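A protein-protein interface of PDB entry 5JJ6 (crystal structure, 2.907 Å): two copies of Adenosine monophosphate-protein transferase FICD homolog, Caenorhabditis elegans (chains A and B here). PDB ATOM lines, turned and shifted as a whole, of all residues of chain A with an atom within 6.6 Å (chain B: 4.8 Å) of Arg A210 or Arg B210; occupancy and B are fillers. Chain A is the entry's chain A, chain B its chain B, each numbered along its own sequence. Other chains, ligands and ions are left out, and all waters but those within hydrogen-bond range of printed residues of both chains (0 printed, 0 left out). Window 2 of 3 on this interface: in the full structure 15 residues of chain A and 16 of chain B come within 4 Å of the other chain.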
ATOM      1  N   GLY A 180      17.992   4.759 -21.497  1.00  0.00           N
ATOM      2  CA  GLY A 180      17.496   3.398 -21.510  1.00  0.00           C
ATOM      3  C   GLY A 180      18.314   2.503 -20.604  1.00  0.00           C
ATOM      4  O   GLY A 180      17.762   1.759 -19.790  1.00  0.00           O
ATOM      5  N   ILE A 205      13.404 -10.880 -18.708  1.00  0.00           N
ATOM      6  CA  ILE A 205      14.280 -10.556 -19.834  1.00  0.00           C
ATOM      7  C   ILE A 205      13.576  -9.593 -20.782  1.00  0.00           C
ATOM      8  O   ILE A 205      14.172  -8.611 -21.246  1.00  0.00           O
ATOM      9  CB  ILE A 205      14.745 -11.813 -20.614  1.00  0.00           C
ATOM     10  CG1 ILE A 205      15.722 -12.622 -19.772  1.00  0.00           C
ATOM     11  CG2 ILE A 205      15.486 -11.432 -21.890  1.00  0.00           C
ATOM     12  CD1 ILE A 205      16.178 -13.882 -20.454  1.00  0.00           C
ATOM     13  N   LEU A 206      12.300  -9.849 -21.042  1.00  0.00           N
ATOM     14  CA  LEU A 206      11.527  -8.939 -21.892  1.00  0.00           C
ATOM     15  C   LEU A 206      11.510  -7.505 -21.328  1.00  0.00           C
ATOM     16  O   LEU A 206      11.658  -6.528 -22.063  1.00  0.00           O
ATOM     17  CB  LEU A 206      10.105  -9.483 -22.054  1.00  0.00           C
ATOM     18  CG  LEU A 206      10.078 -10.750 -22.914  1.00  0.00           C
ATOM     19  CD1 LEU A 206       8.698 -11.369 -22.989  1.00  0.00           C
ATOM     20  CD2 LEU A 206      10.585 -10.433 -24.311  1.00  0.00           C
ATOM     21  N   GLU A 207      11.368  -7.387 -20.014  1.00  0.00           N
ATOM     22  CA  GLU A 207      11.304  -6.085 -19.371  1.00  0.00           C
ATOM     23  C   GLU A 207      12.655  -5.398 -19.403  1.00  0.00           C
ATOM     24  O   GLU A 207      12.734  -4.180 -19.610  1.00  0.00           O
ATOM     25  CB  GLU A 207      10.802  -6.216 -17.932  1.00  0.00           C
ATOM     26  CG  GLU A 207       9.287  -6.444 -17.844  1.00  0.00           C
ATOM     27  CD  GLU A 207       8.501  -5.465 -18.703  1.00  0.00           C
ATOM     28  OE1 GLU A 207       7.820  -5.918 -19.658  1.00  0.00           O
ATOM     29  OE2 GLU A 207       8.584  -4.244 -18.432  1.00  0.00           O
ATOM     30  N   MET A 208      13.720  -6.176 -19.209  1.00  0.00           N
ATOM     31  CA  MET A 208      15.055  -5.617 -19.345  1.00  0.00           C
ATOM     32  C   MET A 208      15.249  -5.057 -20.728  1.00  0.00           C
ATOM     33  O   MET A 208      15.733  -3.943 -20.865  1.00  0.00           O
ATOM     34  CB  MET A 208      16.137  -6.643 -19.065  1.00  0.00           C
ATOM     35  CG  MET A 208      16.522  -6.736 -17.609  1.00  0.00           C
ATOM     36  SD  MET A 208      18.015  -7.721 -17.375  1.00  0.00           S
ATOM     37  CE  MET A 208      17.510  -9.267 -18.149  1.00  0.00           C
ATOM     38  N   HIS A 209      14.843  -5.790 -21.755  1.00  0.00           N
ATOM     39  CA  HIS A 209      15.014  -5.244 -23.087  1.00  0.00           C
ATOM     40  C   HIS A 209      14.147  -4.008 -23.281  1.00  0.00           C
ATOM     41  O   HIS A 209      14.527  -3.079 -23.995  1.00  0.00           O
ATOM     42  CB  HIS A 209      14.695  -6.264 -24.167  1.00  0.00           C
ATOM     43  CG  HIS A 209      14.971  -5.756 -25.546  1.00  0.00           C
ATOM     44  ND1 HIS A 209      13.976  -5.337 -26.400  1.00  0.00           N
ATOM     45  CD2 HIS A 209      16.139  -5.558 -26.203  1.00  0.00           C
ATOM     46  CE1 HIS A 209      14.516  -4.924 -27.532  1.00  0.00           C
ATOM     47  NE2 HIS A 209      15.828  -5.047 -27.439  1.00  0.00           N
ATOM     48  N   ARG A 210      12.982  -3.999 -22.639  1.00  0.00           N
ATOM     49  CA  ARG A 210      12.037  -2.908 -22.827  1.00  0.00           C
ATOM     50  C   ARG A 210      12.602  -1.625 -22.261  1.00  0.00           C
ATOM     51  O   ARG A 210      12.484  -0.569 -22.875  1.00  0.00           O
ATOM     52  CB  ARG A 210      10.691  -3.229 -22.164  1.00  0.00           C
ATOM     53  CG  ARG A 210       9.656  -2.089 -22.213  1.00  0.00           C
ATOM     54  CD  ARG A 210       9.351  -1.669 -23.641  1.00  0.00           C
ATOM     55  NE  ARG A 210       8.414  -0.550 -23.726  1.00  0.00           N
ATOM     56  CZ  ARG A 210       8.002  -0.010 -24.874  1.00  0.00           C
ATOM     57  NH1 ARG A 210       8.449  -0.487 -26.032  1.00  0.00           N
ATOM     58  NH2 ARG A 210       7.139   1.002 -24.870  1.00  0.00           N
ATOM     59  N   ARG A 211      13.290  -1.724 -21.131  1.00  0.00           N
ATOM     60  CA  ARG A 211      13.899  -0.534 -20.561  1.00  0.00           C
ATOM     61  C   ARG A 211      15.196  -0.186 -21.288  1.00  0.00           C
ATOM     62  O   ARG A 211      15.467   0.989 -21.538  1.00  0.00           O
ATOM     63  CB  ARG A 211      14.151  -0.722 -19.067  1.00  0.00           C
ATOM     64  CG  ARG A 211      12.896  -0.627 -18.231  1.00  0.00           C
ATOM     65  CD  ARG A 211      13.129  -1.084 -16.810  1.00  0.00           C
ATOM     66  NE  ARG A 211      12.002  -0.791 -15.923  1.00  0.00           N
ATOM     67  CZ  ARG A 211      10.864  -1.488 -15.896  1.00  0.00           C
ATOM     68  NH1 ARG A 211      10.685  -2.523 -16.715  1.00  0.00           N
ATOM     69  NH2 ARG A 211       9.895  -1.147 -15.054  1.00  0.00           N
ATOM     70  N   VAL A 212      15.957  -1.201 -21.689  1.00  0.00           N
ATOM     71  CA  VAL A 212      17.187  -0.965 -22.418  1.00  0.00           C
ATOM     72  C   VAL A 212      16.893  -0.117 -23.642  1.00  0.00           C
ATOM     73  O   VAL A 212      17.473   0.954 -23.817  1.00  0.00           O
ATOM     74  CB  VAL A 212      17.858  -2.284 -22.893  1.00  0.00           C
ATOM     75  CG1 VAL A 212      18.855  -2.001 -24.020  1.00  0.00           C
ATOM     76  CG2 VAL A 212      18.556  -2.987 -21.759  1.00  0.00           C
ATOM     77  N   LEU A 213      15.929  -0.550 -24.445  1.00  0.00           N
ATOM     78  CA  LEU A 213      15.739   0.067 -25.748  1.00  0.00           C
ATOM     79  C   LEU A 213      14.563   1.030 -25.816  1.00  0.00           C
ATOM     80  O   LEU A 213      14.381   1.705 -26.825  1.00  0.00           O
ATOM     81  CB  LEU A 213      15.540  -1.019 -26.805  1.00  0.00           C
ATOM     82  CG  LEU A 213      16.139  -0.737 -28.172  1.00  0.00           C
ATOM     83  CD1 LEU A 213      17.590  -1.170 -28.140  1.00  0.00           C
ATOM     84  CD2 LEU A 213      15.378  -1.461 -29.253  1.00  0.00           C
ATOM     85  N   GLY A 214      13.786   1.105 -24.740  1.00  0.00           N
ATOM     86  CA  GLY A 214      12.554   1.877 -24.737  1.00  0.00           C
ATOM     87  C   GLY A 214      12.623   3.276 -25.321  1.00  0.00           C
ATOM     88  O   GLY A 214      11.967   3.575 -26.309  1.00  0.00           O
ATOM     89  N   ASN A 215      13.479   4.113 -24.759  1.00  0.00           N
ATOM     90  CA  ASN A 215      13.586   5.482 -25.212  1.00  0.00           C
ATOM     91  C   ASN A 215      14.100   5.582 -26.643  1.00  0.00           C
ATOM     92  O   ASN A 215      13.608   6.399 -27.417  1.00  0.00           O
ATOM     93  CB  ASN A 215      14.503   6.257 -24.277  1.00  0.00           C
ATOM     94  CG  ASN A 215      14.073   6.164 -22.839  1.00  0.00           C
ATOM     95  OD1 ASN A 215      14.468   5.251 -22.108  1.00  0.00           O
ATOM     96  ND2 ASN A 215      13.270   7.126 -22.409  1.00  0.00           N
ATOM     97  N   ASP A 217      14.057   3.241 -29.149  1.00  0.00           N
ATOM     98  CA  ASP A 217      13.234   2.618 -30.188  1.00  0.00           C
ATOM     99  C   ASP A 217      11.964   1.968 -29.599  1.00  0.00           C
ATOM    100  O   ASP A 217      11.871   0.745 -29.483  1.00  0.00           O
ATOM    101  CB  ASP A 217      14.076   1.594 -30.959  1.00  0.00           C
ATOM    102  CG  ASP A 217      13.487   1.244 -32.314  1.00  0.00           C
ATOM    103  OD1 ASP A 217      12.326   1.625 -32.594  1.00  0.00           O
ATOM    104  OD2 ASP A 217      14.196   0.586 -33.107  1.00  0.00           O
ATOM    105  N   PRO A 218      10.959   2.789 -29.272  1.00  0.00           N
ATOM    106  CA  PRO A 218       9.814   2.312 -28.485  1.00  0.00           C
ATOM    107  C   PRO A 218       9.000   1.208 -29.160  1.00  0.00           C
ATOM    108  O   PRO A 218       8.473   0.346 -28.456  1.00  0.00           O
ATOM    109  CB  PRO A 218       8.957   3.574 -28.307  1.00  0.00           C
ATOM    110  CG  PRO A 218       9.884   4.716 -28.560  1.00  0.00           C
ATOM    111  CD  PRO A 218      10.855   4.222 -29.587  1.00  0.00           C
ATOM    112  N   VAL A 219       8.907   1.223 -30.486  1.00  0.00           N
ATOM    113  CA  VAL A 219       8.143   0.197 -31.190  1.00  0.00           C
ATOM    114  C   VAL A 219       8.771  -1.201 -31.033  1.00  0.00           C
ATOM    115  O   VAL A 219       8.053  -2.205 -30.946  1.00  0.00           O
ATOM    116  CB  VAL A 219       7.998   0.529 -32.695  1.00  0.00           C
ATOM    117  CG1 VAL A 219       7.042   1.696 -32.898  1.00  0.00           C
ATOM    118  CG2 VAL A 219       9.344   0.844 -33.305  1.00  0.00           C
ATOM    119  N   GLU A 220      10.104  -1.264 -30.964  1.00  0.00           N
ATOM    120  CA  GLU A 220      10.798  -2.547 -30.902  1.00  0.00           C
ATOM    121  C   GLU A 220      11.174  -3.000 -29.493  1.00  0.00           C
ATOM    122  O   GLU A 220      11.457  -4.176 -29.277  1.00  0.00           O
ATOM    123  CB  GLU A 220      12.065  -2.498 -31.755  1.00  0.00           C
ATOM    124  CG  GLU A 220      11.818  -2.363 -33.251  1.00  0.00           C
ATOM    125  CD  GLU A 220      11.379  -3.672 -33.902  1.00  0.00           C
ATOM    126  OE1 GLU A 220      11.231  -4.688 -33.181  1.00  0.00           O
ATOM    127  OE2 GLU A 220      11.201  -3.688 -35.141  1.00  0.00           O
ATOM    128  N   ALA A 221      11.147  -2.087 -28.529  1.00  0.00           N
ATOM    129  CA  ALA A 221      11.594  -2.411 -27.177  1.00  0.00           C
ATOM    130  C   ALA A 221      10.669  -3.439 -26.506  1.00  0.00           C
ATOM    131  O   ALA A 221       9.442  -3.333 -26.578  1.00  0.00           O
ATOM    132  CB  ALA A 221      11.690  -1.149 -26.336  1.00  0.00           C
ATOM    133  N   GLY A 222      11.285  -4.438 -25.874  1.00  0.00           N
ATOM    134  CA  GLY A 222      10.588  -5.517 -25.195  1.00  0.00           C
ATOM    135  C   GLY A 222       9.813  -6.455 -26.108  1.00  0.00           C
ATOM    136  O   GLY A 222       8.878  -7.136 -25.669  1.00  0.00           O
ATOM    137  N   ARG A 223      10.189  -6.491 -27.382  1.00  0.00           N
ATOM    138  CA  ARG A 223       9.451  -7.285 -28.351  1.00  0.00           C
ATOM    139  C   ARG A 223      10.343  -8.214 -29.166  1.00  0.00           C
ATOM    140  O   ARG A 223      11.436  -7.843 -29.590  1.00  0.00           O
ATOM    141  CB  ARG A 223       8.639  -6.374 -29.274  1.00  0.00           C
ATOM    142  CG  ARG A 223       9.095  -6.299 -30.722  1.00  0.00           C
ATOM    143  CD  ARG A 223       7.920  -5.834 -31.569  1.00  0.00           C
ATOM    144  NE  ARG A 223       8.284  -5.474 -32.934  1.00  0.00           N
ATOM    145  CZ  ARG A 223       7.423  -4.982 -33.821  1.00  0.00           C
ATOM    146  NH1 ARG A 223       6.148  -4.805 -33.485  1.00  0.00           N
ATOM    147  NH2 ARG A 223       7.834  -4.671 -35.045  1.00  0.00           N
ATOM    148  N   PHE A 280      15.929 -10.179 -30.233  1.00  0.00           N
ATOM    149  CA  PHE A 280      15.377  -8.871 -30.545  1.00  0.00           C
ATOM    150  C   PHE A 280      15.919  -8.339 -31.864  1.00  0.00           C
ATOM    151  O   PHE A 280      16.985  -8.754 -32.312  1.00  0.00           O
ATOM    152  CB  PHE A 280      15.684  -7.901 -29.416  1.00  0.00           C
ATOM    153  CG  PHE A 280      15.388  -8.450 -28.064  1.00  0.00           C
ATOM    154  CD1 PHE A 280      14.080  -8.597 -27.633  1.00  0.00           C
ATOM    155  CD2 PHE A 280      16.418  -8.826 -27.221  1.00  0.00           C
ATOM    156  CE1 PHE A 280      13.795  -9.118 -26.374  1.00  0.00           C
ATOM    157  CE2 PHE A 280      16.148  -9.343 -25.960  1.00  0.00           C
ATOM    158  CZ  PHE A 280      14.829  -9.492 -25.534  1.00  0.00           C
ATOM    159  N   THR A 287      21.638  -6.115 -23.657  1.00  0.00           N
ATOM    160  CA  THR A 287      20.891  -6.986 -22.756  1.00  0.00           C
ATOM    161  C   THR A 287      21.733  -8.198 -22.319  1.00  0.00           C
ATOM    162  O   THR A 287      21.695  -8.588 -21.158  1.00  0.00           O
ATOM    163  CB  THR A 287      19.570  -7.491 -23.400  1.00  0.00           C
ATOM    164  OG1 THR A 287      18.867  -6.396 -23.995  1.00  0.00           O
ATOM    165  CG2 THR A 287      18.670  -8.161 -22.356  1.00  0.00           C
ATOM    166  N   LEU B 206      -4.791   2.967 -27.418  1.00  0.00           N
ATOM    167  CA  LEU B 206      -3.576   2.460 -26.797  1.00  0.00           C
ATOM    168  C   LEU B 206      -2.346   2.702 -27.660  1.00  0.00           C
ATOM    169  O   LEU B 206      -1.283   3.028 -27.137  1.00  0.00           O
ATOM    170  CB  LEU B 206      -3.706   0.970 -26.490  1.00  0.00           C
ATOM    171  CG  LEU B 206      -4.674   0.674 -25.351  1.00  0.00           C
ATOM    172  CD1 LEU B 206      -4.814  -0.820 -25.125  1.00  0.00           C
ATOM    173  CD2 LEU B 206      -4.226   1.384 -24.084  1.00  0.00           C
ATOM    174  N   GLU B 207      -2.489   2.530 -28.972  1.00  0.00           N
ATOM    175  CA  GLU B 207      -1.369   2.702 -29.895  1.00  0.00           C
ATOM    176  C   GLU B 207      -0.987   4.151 -29.999  1.00  0.00           C
ATOM    177  O   GLU B 207       0.200   4.489 -30.083  1.00  0.00           O
ATOM    178  CB  GLU B 207      -1.691   2.154 -31.284  1.00  0.00           C
ATOM    179  CG  GLU B 207      -1.574   0.649 -31.382  1.00  0.00           C
ATOM    180  CD  GLU B 207      -0.272   0.139 -30.794  1.00  0.00           C
ATOM    181  OE1 GLU B 207       0.808   0.521 -31.312  1.00  0.00           O
ATOM    182  OE2 GLU B 207      -0.339  -0.636 -29.808  1.00  0.00           O
ATOM    183  N   MET B 208      -1.992   5.012 -30.010  1.00  0.00           N
ATOM    184  CA  MET B 208      -1.711   6.431 -29.983  1.00  0.00           C
ATOM    185  C   MET B 208      -0.961   6.813 -28.709  1.00  0.00           C
ATOM    186  O   MET B 208       0.005   7.570 -28.777  1.00  0.00           O
ATOM    187  CB  MET B 208      -2.990   7.240 -30.126  1.00  0.00           C
ATOM    188  CG  MET B 208      -3.387   7.436 -31.572  1.00  0.00           C
ATOM    189  SD  MET B 208      -4.708   8.642 -31.756  1.00  0.00           S
ATOM    190  CE  MET B 208      -5.974   7.943 -30.694  1.00  0.00           C
ATOM    191  N   HIS B 209      -1.382   6.289 -27.558  1.00  0.00           N
ATOM    192  CA  HIS B 209      -0.689   6.608 -26.308  1.00  0.00           C
ATOM    193  C   HIS B 209       0.729   6.039 -26.282  1.00  0.00           C
ATOM    194  O   HIS B 209       1.654   6.638 -25.730  1.00  0.00           O
ATOM    195  CB  HIS B 209      -1.464   6.083 -25.103  1.00  0.00           C
ATOM    196  CG  HIS B 209      -0.857   6.458 -23.786  1.00  0.00           C
ATOM    197  ND1 HIS B 209      -0.113   5.575 -23.030  1.00  0.00           N
ATOM    198  CD2 HIS B 209      -0.888   7.616 -23.085  1.00  0.00           C
ATOM    199  CE1 HIS B 209       0.292   6.176 -21.926  1.00  0.00           C
ATOM    200  NE2 HIS B 209      -0.168   7.416 -21.933  1.00  0.00           N
ATOM    201  N   ARG B 210       0.888   4.874 -26.892  1.00  0.00           N
ATOM    202  CA  ARG B 210       2.154   4.164 -26.888  1.00  0.00           C
ATOM    203  C   ARG B 210       3.119   4.995 -27.708  1.00  0.00           C
ATOM    204  O   ARG B 210       4.298   5.080 -27.396  1.00  0.00           O
ATOM    205  CB  ARG B 210       1.986   2.744 -27.446  1.00  0.00           C
ATOM    206  CG  ARG B 210       3.258   1.940 -27.519  1.00  0.00           C
ATOM    207  CD  ARG B 210       3.013   0.427 -27.541  1.00  0.00           C
ATOM    208  NE  ARG B 210       4.174  -0.271 -26.974  1.00  0.00           N
ATOM    209  CZ  ARG B 210       4.137  -1.036 -25.882  1.00  0.00           C
ATOM    210  NH1 ARG B 210       2.982  -1.235 -25.245  1.00  0.00           N
ATOM    211  NH2 ARG B 210       5.252  -1.614 -25.433  1.00  0.00           N
ATOM    212  N   ARG B 211       2.617   5.648 -28.747  1.00  0.00           N
ATOM    213  CA  ARG B 211       3.487   6.540 -29.501  1.00  0.00           C
ATOM    214  C   ARG B 211       3.672   7.929 -28.842  1.00  0.00           C
ATOM    215  O   ARG B 211       4.754   8.523 -28.928  1.00  0.00           O
ATOM    216  CB  ARG B 211       2.974   6.652 -30.927  1.00  0.00           C
ATOM    217  CG  ARG B 211       3.300   5.383 -31.688  1.00  0.00           C
ATOM    218  CD  ARG B 211       2.614   5.267 -33.024  1.00  0.00           C
ATOM    219  NE  ARG B 211       3.153   4.145 -33.788  1.00  0.00           N
ATOM    220  CZ  ARG B 211       2.849   2.871 -33.559  1.00  0.00           C
ATOM    221  NH1 ARG B 211       1.997   2.559 -32.588  1.00  0.00           N
ATOM    222  NH2 ARG B 211       3.391   1.909 -34.300  1.00  0.00           N
ATOM    223  N   VAL B 212       2.632   8.440 -28.187  1.00  0.00           N
ATOM    224  CA  VAL B 212       2.712   9.713 -27.462  1.00  0.00           C
ATOM    225  C   VAL B 212       3.812   9.659 -26.410  1.00  0.00           C
ATOM    226  O   VAL B 212       4.611  10.587 -26.290  1.00  0.00           O
ATOM    227  CB  VAL B 212       1.371  10.085 -26.779  1.00  0.00           C
ATOM    228  CG1 VAL B 212       1.587  11.119 -25.694  1.00  0.00           C
ATOM    229  CG2 VAL B 212       0.390  10.619 -27.790  1.00  0.00           C
ATOM    230  N   LEU B 213       3.824   8.591 -25.617  1.00  0.00           N
ATOM    231  CA  LEU B 213       4.740   8.510 -24.478  1.00  0.00           C
ATOM    232  C   LEU B 213       5.937   7.591 -24.712  1.00  0.00           C
ATOM    233  O   LEU B 213       6.791   7.462 -23.838  1.00  0.00           O
ATOM    234  CB  LEU B 213       4.007   8.045 -23.219  1.00  0.00           C
ATOM    235  CG  LEU B 213       3.309   9.123 -22.402  1.00  0.00           C
ATOM    236  CD1 LEU B 213       3.091   8.603 -21.009  1.00  0.00           C
ATOM    237  CD2 LEU B 213       4.142  10.392 -22.396  1.00  0.00           C
ATOM    238  N   GLY B 214       5.974   6.933 -25.868  1.00  0.00           N
ATOM    239  CA  GLY B 214       7.004   5.947 -26.163  1.00  0.00           C
ATOM    240  C   GLY B 214       8.441   6.355 -25.858  1.00  0.00           C
ATOM    241  O   GLY B 214       9.147   5.673 -25.110  1.00  0.00           O
ATOM    242  N   PRO B 218       8.926   5.165 -21.773  1.00  0.00           N
ATOM    243  CA  PRO B 218       8.593   3.897 -22.437  1.00  0.00           C
ATOM    244  C   PRO B 218       7.927   2.852 -21.539  1.00  0.00           C
ATOM    245  O   PRO B 218       7.106   2.074 -22.014  1.00  0.00           O
ATOM    246  CB  PRO B 218       9.956   3.403 -22.935  1.00  0.00           C
ATOM    247  CG  PRO B 218      10.939   4.091 -22.084  1.00  0.00           C
ATOM    248  CD  PRO B 218      10.372   5.430 -21.790  1.00  0.00           C
ATOM    249  N   ALA B 221       4.103   3.710 -21.530  1.00  0.00           N
ATOM    250  CA  ALA B 221       3.411   3.936 -22.803  1.00  0.00           C
ATOM    251  C   ALA B 221       2.499   2.795 -23.252  1.00  0.00           C
ATOM    252  O   ALA B 221       2.887   1.632 -23.259  1.00  0.00           O
ATOM    253  CB  ALA B 221       4.428   4.224 -23.892  1.00  0.00           C
ATOM    254  N   GLY B 222       1.287   3.161 -23.657  1.00  0.00           N
ATOM    255  CA  GLY B 222       0.286   2.208 -24.105  1.00  0.00           C
ATOM    256  C   GLY B 222      -0.154   1.304 -22.971  1.00  0.00           C
ATOM    257  O   GLY B 222      -0.741   0.234 -23.185  1.00  0.00           O
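Arg A210 touches its own counterpart, Arg B210.
Arg A210 touches Pro B218, but with the chains exchanged Pro A218 does not touch Arg B210 (4.6 Å).
Gly B214 touches its own counterpart, Gly A214.
Gly A214 touches Pro B218, and with the chains exchanged Pro A218 touches Gly B214.
Positions printed for both chains: 206, 207, 208, 209, 210, 211, 212, 213, 214, 218, 221 and 222.
Along chain A the printed residues that touch a printed residue of chain B span positions 210 to 219.
Among the printed residues, 7 pairs touch across the chains.
Among the printed residues, no Asp or Glu carboxylate lies within 4 Å of a Lys or Arg side-chain nitrogen of the other chain.
Gly A214 touches Gly B214.
CA of Gly A214 touches CB of Pro B218 (3.5 Å).
Pro B218 touches Asn A215.
Gly B214 touches Pro A218.
Arg B211 touches Val A219 (NH2 to CG1, 3.9 Å).
The guanidinium group (NH2) of Arg A210 sits at hydrogen-bond distance from the backbone carbonyl oxygen (O) of Pro B218 (3.1 Å).
The guanidinium group (NH2) of Arg A210 lies close to the guanidinium group (NH2) of Arg B210 (3.3 Å).
Arg A210 touches two residues of chain B.
Val A212 touches none of the printed residues of chain B.
Of the printed residues of chain B, Gly A214 touches Gly B214 and Pro B218.
Of chain A, only Arg A210 comes within 4 Å of Arg B210.
Of the printed residues of chain A, Pro B218 touches Arg A210 (3.1 Å), Gly A214 (3.5 Å) and Asn A215 (3.4 Å).
The nearest printed residue of chain B that does not touch Gly A214 is Leu B213 (6.9 Å).
The guanidinium group (NH1) of Arg A210 sits at hydrogen-bond distance from the backbone carbonyl oxygen (O) of Pro A218 (2.6 Å).
O of Ala A221 is in hydrogen-bond range of NH1 of Arg A210, 3.1 Å away.
The guanidinium group of Arg B211 is in salt-bridge range of the side-chain carboxylate of Glu B207, 2.7 Å away.
NH1 of Arg B210 lies within hydrogen-bond range of O of Ala B221, 3.5 Å away.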
